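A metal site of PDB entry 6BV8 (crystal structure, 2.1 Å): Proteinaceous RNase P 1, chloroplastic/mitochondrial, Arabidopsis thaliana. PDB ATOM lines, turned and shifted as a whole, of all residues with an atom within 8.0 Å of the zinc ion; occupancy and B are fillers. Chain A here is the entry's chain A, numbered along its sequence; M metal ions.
SG of Cys 276 sits close to N of Glu 278 (3.5 Å).
The backbone NH of Cys 494 lies within hydrogen-bond range of the backbone carbonyl oxygen of Lys 263, at 2.8 Å.
The backbone NH of Cys 275 sits close to the side-chain sulfur of Cys 273 (3.5 Å).
The backbone carbonyl oxygen of Glu 278 sits at hydrogen-bond distance from the backbone NH of Cys 273.
N of Cys 273 sits close to SD of Met 267, at 3.6 Å.
Of the 23 residues printed, 4 come within 4 Å of the zinc ion.
The zinc ion is bound by a ring nitrogen (NE2) of His 477 (2.1 Å), the side-chain sulfur (SG) of Cys 276 (2.3 Å), the side-chain sulfur (SG) of Cys 494 (2.3 Å) and the side-chain sulfur (SG) of Cys 273 (2.3 Å).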
ATOM      1  N   ASN A 261      21.205  11.822  23.004  1.00  0.00           N
ATOM      2  CA  ASN A 261      20.932  12.704  21.850  1.00  0.00           C
ATOM      3  C   ASN A 261      19.539  13.294  22.009  1.00  0.00           C
ATOM      4  O   ASN A 261      18.551  12.562  21.972  1.00  0.00           O
ATOM      5  CB  ASN A 261      20.971  11.951  20.515  1.00  0.00           C
ATOM      6  CG  ASN A 261      22.373  11.528  20.107  1.00  0.00           C
ATOM      7  OD1 ASN A 261      23.371  12.107  20.562  1.00  0.00           O
ATOM      8  ND2 ASN A 261      22.452  10.509  19.257  1.00  0.00           N
ATOM      9  N   LYS A 263      16.909  16.073  20.616  1.00  0.00           N
ATOM     10  CA  LYS A 263      16.491  17.030  19.585  1.00  0.00           C
ATOM     11  C   LYS A 263      15.043  17.416  19.739  1.00  0.00           C
ATOM     12  O   LYS A 263      14.198  16.564  20.061  1.00  0.00           O
ATOM     13  CB  LYS A 263      16.676  16.453  18.174  1.00  0.00           C
ATOM     14  CG  LYS A 263      18.007  15.770  17.910  1.00  0.00           C
ATOM     15  CD  LYS A 263      19.237  16.663  18.101  1.00  0.00           C
ATOM     16  CE  LYS A 263      20.448  15.821  18.507  1.00  0.00           C
ATOM     17  NZ  LYS A 263      21.632  16.668  18.816  1.00  0.00           N
ATOM     18  N   THR A 265      11.855  18.200  17.602  1.00  0.00           N
ATOM     19  CA  THR A 265      11.442  17.552  16.368  1.00  0.00           C
ATOM     20  C   THR A 265       9.905  17.503  16.313  1.00  0.00           C
ATOM     21  O   THR A 265       9.221  18.187  17.083  1.00  0.00           O
ATOM     22  CB  THR A 265      12.118  16.166  16.215  1.00  0.00           C
ATOM     23  OG1 THR A 265      11.847  15.634  14.919  1.00  0.00           O
ATOM     24  CG2 THR A 265      11.659  15.170  17.269  1.00  0.00           C
ATOM     25  N   GLU A 266       9.378  16.749  15.347  1.00  0.00           N
ATOM     26  CA  GLU A 266       7.947  16.587  15.145  1.00  0.00           C
ATOM     27  C   GLU A 266       7.685  15.155  14.785  1.00  0.00           C
ATOM     28  O   GLU A 266       8.618  14.403  14.449  1.00  0.00           O
ATOM     29  CB  GLU A 266       7.472  17.475  14.006  1.00  0.00           C
ATOM     30  CG  GLU A 266       7.616  18.962  14.281  1.00  0.00           C
ATOM     31  CD  GLU A 266       7.501  19.824  13.041  1.00  0.00           C
ATOM     32  OE1 GLU A 266       7.501  19.267  11.899  1.00  0.00           O
ATOM     33  OE2 GLU A 266       7.427  21.064  13.217  1.00  0.00           O
ATOM     34  N   MET A 267       6.420  14.781  14.852  1.00  0.00           N
ATOM     35  CA  MET A 267       5.969  13.497  14.356  1.00  0.00           C
ATOM     36  C   MET A 267       5.293  13.752  13.034  1.00  0.00           C
ATOM     37  O   MET A 267       4.631  14.780  12.854  1.00  0.00           O
ATOM     38  CB  MET A 267       4.988  12.850  15.321  1.00  0.00           C
ATOM     39  CG  MET A 267       5.515  12.698  16.727  1.00  0.00           C
ATOM     40  SD  MET A 267       6.844  11.492  16.861  1.00  0.00           S
ATOM     41  CE  MET A 267       8.058  12.587  17.600  1.00  0.00           C
ATOM     42  N   VAL A 272       5.430   8.838  13.321  1.00  0.00           N
ATOM     43  CA  VAL A 272       6.827   8.484  13.180  1.00  0.00           C
ATOM     44  C   VAL A 272       7.634   9.736  13.495  1.00  0.00           C
ATOM     45  O   VAL A 272       7.342  10.817  12.967  1.00  0.00           O
ATOM     46  CB  VAL A 272       7.146   7.944  11.781  1.00  0.00           C
ATOM     47  CG1 VAL A 272       8.634   7.686  11.633  1.00  0.00           C
ATOM     48  CG2 VAL A 272       6.362   6.656  11.528  1.00  0.00           C
ATOM     49  N   CYS A 273       8.625   9.592  14.371  1.00  0.00           N
ATOM     50  CA  CYS A 273       9.517  10.687  14.746  1.00  0.00           C
ATOM     51  C   CYS A 273      10.456  11.001  13.589  1.00  0.00           C
ATOM     52  O   CYS A 273      11.128  10.112  13.056  1.00  0.00           O
ATOM     53  CB  CYS A 273      10.321  10.297  15.999  1.00  0.00           C
ATOM     54  SG  CYS A 273      11.610  11.445  16.567  1.00  0.00           S
ATOM     55  N   LYS A 274      10.479  12.262  13.212  1.00  0.00           N
ATOM     56  CA  LYS A 274      11.302  12.708  12.096  1.00  0.00           C
ATOM     57  C   LYS A 274      12.785  12.721  12.428  1.00  0.00           C
ATOM     58  O   LYS A 274      13.609  12.680  11.528  1.00  0.00           O
ATOM     59  CB  LYS A 274      10.880  14.097  11.645  1.00  0.00           C
ATOM     60  CG  LYS A 274       9.499  14.121  11.006  1.00  0.00           C
ATOM     61  CD  LYS A 274       9.141  15.550  10.654  1.00  0.00           C
ATOM     62  CE  LYS A 274       7.736  15.648  10.115  1.00  0.00           C
ATOM     63  NZ  LYS A 274       7.332  17.072  10.065  1.00  0.00           N
ATOM     64  N   CYS A 275      13.114  12.788  13.720  1.00  0.00           N
ATOM     65  CA  CYS A 275      14.485  12.622  14.153  1.00  0.00           C
ATOM     66  C   CYS A 275      14.891  11.145  14.110  1.00  0.00           C
ATOM     67  O   CYS A 275      15.752  10.790  13.308  1.00  0.00           O
ATOM     68  CB  CYS A 275      14.705  13.222  15.538  1.00  0.00           C
ATOM     69  SG  CYS A 275      16.448  13.608  15.768  1.00  0.00           S
ATOM     70  N   CYS A 276      14.293  10.277  14.921  1.00  0.00           N
ATOM     71  CA  CYS A 276      14.780   8.888  15.028  1.00  0.00           C
ATOM     72  C   CYS A 276      14.007   7.814  14.238  1.00  0.00           C
ATOM     73  O   CYS A 276      14.411   6.671  14.231  1.00  0.00           O
ATOM     74  CB  CYS A 276      14.860   8.439  16.491  1.00  0.00           C
ATOM     75  SG  CYS A 276      13.293   8.032  17.310  1.00  0.00           S
ATOM     76  N   LYS A 277      12.882   8.175  13.606  1.00  0.00           N
ATOM     77  CA  LYS A 277      12.080   7.219  12.843  1.00  0.00           C
ATOM     78  C   LYS A 277      11.407   6.154  13.678  1.00  0.00           C
ATOM     79  O   LYS A 277      10.960   5.138  13.131  1.00  0.00           O
ATOM     80  CB  LYS A 277      12.902   6.552  11.702  1.00  0.00           C
ATOM     81  CG  LYS A 277      13.661   7.528  10.800  1.00  0.00           C
ATOM     82  CD  LYS A 277      12.713   8.462  10.040  1.00  0.00           C
ATOM     83  CE  LYS A 277      13.479   9.523   9.257  1.00  0.00           C
ATOM     84  NZ  LYS A 277      14.280  10.409  10.147  1.00  0.00           N
ATOM     85  N   GLU A 278      11.321   6.343  14.999  1.00  0.00           N
ATOM     86  CA  GLU A 278      10.514   5.418  15.803  1.00  0.00           C
ATOM     87  C   GLU A 278       9.002   5.719  15.566  1.00  0.00           C
ATOM     88  O   GLU A 278       8.599   6.879  15.489  1.00  0.00           O
ATOM     89  CB  GLU A 278      10.868   5.509  17.279  1.00  0.00           C
ATOM     90  CG  GLU A 278      10.012   4.584  18.128  1.00  0.00           C
ATOM     91  CD  GLU A 278      10.565   4.274  19.495  1.00  0.00           C
ATOM     92  OE1 GLU A 278      11.783   4.445  19.726  1.00  0.00           O
ATOM     93  OE2 GLU A 278       9.763   3.833  20.341  1.00  0.00           O
ATOM     94  N   LYS A 279       8.205   4.663  15.450  1.00  0.00           N
ATOM     95  CA  LYS A 279       6.752   4.789  15.319  1.00  0.00           C
ATOM     96  C   LYS A 279       6.166   4.782  16.719  1.00  0.00           C
ATOM     97  O   LYS A 279       6.274   3.808  17.427  1.00  0.00           O
ATOM     98  CB  LYS A 279       6.159   3.641  14.503  1.00  0.00           C
ATOM     99  CG  LYS A 279       4.733   3.922  14.036  1.00  0.00           C
ATOM    100  CD  LYS A 279       4.118   2.694  13.386  1.00  0.00           C
ATOM    101  CE  LYS A 279       2.605   2.785  13.287  1.00  0.00           C
ATOM    102  NZ  LYS A 279       2.160   3.918  12.420  1.00  0.00           N
ATOM    103  N   LEU A 280       5.539   5.891  17.091  1.00  0.00           N
ATOM    104  CA  LEU A 280       4.917   6.007  18.395  1.00  0.00           C
ATOM    105  C   LEU A 280       3.747   5.047  18.467  1.00  0.00           C
ATOM    106  O   LEU A 280       3.200   4.667  17.434  1.00  0.00           O
ATOM    107  CB  LEU A 280       4.460   7.449  18.651  1.00  0.00           C
ATOM    108  CG  LEU A 280       5.555   8.515  18.778  1.00  0.00           C
ATOM    109  CD1 LEU A 280       4.943   9.741  19.419  1.00  0.00           C
ATOM    110  CD2 LEU A 280       6.748   8.062  19.599  1.00  0.00           C
ATOM    111  N   THR A 475      14.149   4.814  24.839  1.00  0.00           N
ATOM    112  CA  THR A 475      13.988   6.097  24.115  1.00  0.00           C
ATOM    113  C   THR A 475      12.735   6.846  24.603  1.00  0.00           C
ATOM    114  O   THR A 475      11.699   6.228  24.849  1.00  0.00           O
ATOM    115  CB  THR A 475      13.893   5.888  22.607  1.00  0.00           C
ATOM    116  OG1 THR A 475      15.044   5.152  22.189  1.00  0.00           O
ATOM    117  CG2 THR A 475      13.842   7.208  21.843  1.00  0.00           C
ATOM    118  N   TRP A 476      12.864   8.168  24.762  1.00  0.00           N
ATOM    119  CA  TRP A 476      11.784   9.009  25.237  1.00  0.00           C
ATOM    120  C   TRP A 476      11.311   9.954  24.149  1.00  0.00           C
ATOM    121  O   TRP A 476      12.134  10.572  23.472  1.00  0.00           O
ATOM    122  CB  TRP A 476      12.213   9.840  26.454  1.00  0.00           C
ATOM    123  CG  TRP A 476      12.343   9.035  27.703  1.00  0.00           C
ATOM    124  CD1 TRP A 476      13.413   8.287  28.085  1.00  0.00           C
ATOM    125  CD2 TRP A 476      11.351   8.870  28.730  1.00  0.00           C
ATOM    126  NE1 TRP A 476      13.157   7.661  29.280  1.00  0.00           N
ATOM    127  CE2 TRP A 476      11.909   8.010  29.709  1.00  0.00           C
ATOM    128  CE3 TRP A 476      10.053   9.369  28.930  1.00  0.00           C
ATOM    129  CZ2 TRP A 476      11.200   7.624  30.867  1.00  0.00           C
ATOM    130  CZ3 TRP A 476       9.353   8.978  30.087  1.00  0.00           C
ATOM    131  CH2 TRP A 476       9.935   8.117  31.033  1.00  0.00           C
ATOM    132  N   HIS A 477       9.991  10.062  24.001  1.00  0.00           N
ATOM    133  CA  HIS A 477       9.386  11.123  23.215  1.00  0.00           C
ATOM    134  C   HIS A 477       8.414  11.917  24.069  1.00  0.00           C
ATOM    135  O   HIS A 477       7.502  11.365  24.681  1.00  0.00           O
ATOM    136  CB  HIS A 477       8.703  10.524  22.010  1.00  0.00           C
ATOM    137  CG  HIS A 477       9.663   9.955  21.026  1.00  0.00           C
ATOM    138  ND1 HIS A 477      10.035   8.625  21.020  1.00  0.00           N
ATOM    139  CD2 HIS A 477      10.349  10.541  20.029  1.00  0.00           C
ATOM    140  CE1 HIS A 477      10.908   8.424  20.062  1.00  0.00           C
ATOM    141  NE2 HIS A 477      11.126   9.574  19.440  1.00  0.00           N
ATOM    142  N   VAL A 478       8.610  13.228  24.097  1.00  0.00           N
ATOM    143  CA  VAL A 478       7.846  14.097  24.998  1.00  0.00           C
ATOM    144  C   VAL A 478       7.155  15.191  24.164  1.00  0.00           C
ATOM    145  O   VAL A 478       7.839  15.977  23.515  1.00  0.00           O
ATOM    146  CB  VAL A 478       8.779  14.720  26.054  1.00  0.00           C
ATOM    147  CG1 VAL A 478       8.023  15.690  26.940  1.00  0.00           C
ATOM    148  CG2 VAL A 478       9.437  13.614  26.883  1.00  0.00           C
ATOM    149  N   TRP A 492       7.950  18.218  19.698  1.00  0.00           N
ATOM    150  CA  TRP A 492       8.263  17.069  20.491  1.00  0.00           C
ATOM    151  C   TRP A 492       9.735  17.064  20.863  1.00  0.00           C
ATOM    152  O   TRP A 492      10.578  17.513  20.094  1.00  0.00           O
ATOM    153  CB  TRP A 492       8.014  15.786  19.694  1.00  0.00           C
ATOM    154  CG  TRP A 492       6.570  15.429  19.515  1.00  0.00           C
ATOM    155  CD1 TRP A 492       5.683  16.007  18.635  1.00  0.00           C
ATOM    156  CD2 TRP A 492       5.843  14.388  20.197  1.00  0.00           C
ATOM    157  NE1 TRP A 492       4.456  15.390  18.746  1.00  0.00           N
ATOM    158  CE2 TRP A 492       4.524  14.398  19.677  1.00  0.00           C
ATOM    159  CE3 TRP A 492       6.184  13.442  21.178  1.00  0.00           C
ATOM    160  CZ2 TRP A 492       3.534  13.499  20.121  1.00  0.00           C
ATOM    161  CZ3 TRP A 492       5.203  12.554  21.623  1.00  0.00           C
ATOM    162  CH2 TRP A 492       3.892  12.595  21.094  1.00  0.00           C
ATOM    163  N   LEU A 493      10.040  16.513  22.028  1.00  0.00           N
ATOM    164  CA  LEU A 493      11.403  16.192  22.396  1.00  0.00           C
ATOM    165  C   LEU A 493      11.710  14.723  22.093  1.00  0.00           C
ATOM    166  O   LEU A 493      10.939  13.823  22.488  1.00  0.00           O
ATOM    167  CB  LEU A 493      11.611  16.494  23.878  1.00  0.00           C
ATOM    168  CG  LEU A 493      13.033  16.878  24.295  1.00  0.00           C
ATOM    169  CD1 LEU A 493      13.413  18.228  23.688  1.00  0.00           C
ATOM    170  CD2 LEU A 493      13.140  16.928  25.819  1.00  0.00           C
ATOM    171  N   CYS A 494      12.812  14.491  21.369  1.00  0.00           N
ATOM    172  CA  CYS A 494      13.318  13.156  21.105  1.00  0.00           C
ATOM    173  C   CYS A 494      14.634  12.969  21.866  1.00  0.00           C
ATOM    174  O   CYS A 494      15.643  13.635  21.566  1.00  0.00           O
ATOM    175  CB  CYS A 494      13.549  12.962  19.619  1.00  0.00           C
ATOM    176  SG  CYS A 494      14.246  11.353  19.210  1.00  0.00           S
ATOM    177  N   ALA A 495      14.615  12.066  22.864  1.00  0.00           N
ATOM    178  CA  ALA A 495      15.768  11.768  23.694  1.00  0.00           C
ATOM    179  C   ALA A 495      16.136  10.304  23.548  1.00  0.00           C
ATOM    180  O   ALA A 495      15.414   9.407  24.020  1.00  0.00           O
ATOM    181  CB  ALA A 495      15.475  12.100  25.133  1.00  0.00           C
ATOM    182  N   LYS A 496      17.250  10.072  22.869  1.00  0.00           N
ATOM    183  CA  LYS A 496      17.707   8.733  22.491  1.00  0.00           C
ATOM    184  C   LYS A 496      19.195   8.557  22.835  1.00  0.00           C
ATOM    185  O   LYS A 496      20.001   9.423  22.532  1.00  0.00           O
ATOM    186  CB  LYS A 496      17.487   8.590  20.993  1.00  0.00           C
ATOM    187  CG  LYS A 496      17.661   7.187  20.433  1.00  0.00           C
ATOM    188  CD  LYS A 496      17.219   7.180  18.965  1.00  0.00           C
ATOM    189  CE  LYS A 496      17.587   5.881  18.267  1.00  0.00           C
ATOM    190  NZ  LYS A 496      17.032   4.720  19.002  1.00  0.00           N
HETATM  191 ZN    ZN M   1      12.647  10.042  18.136  1.00  0.00          ZN
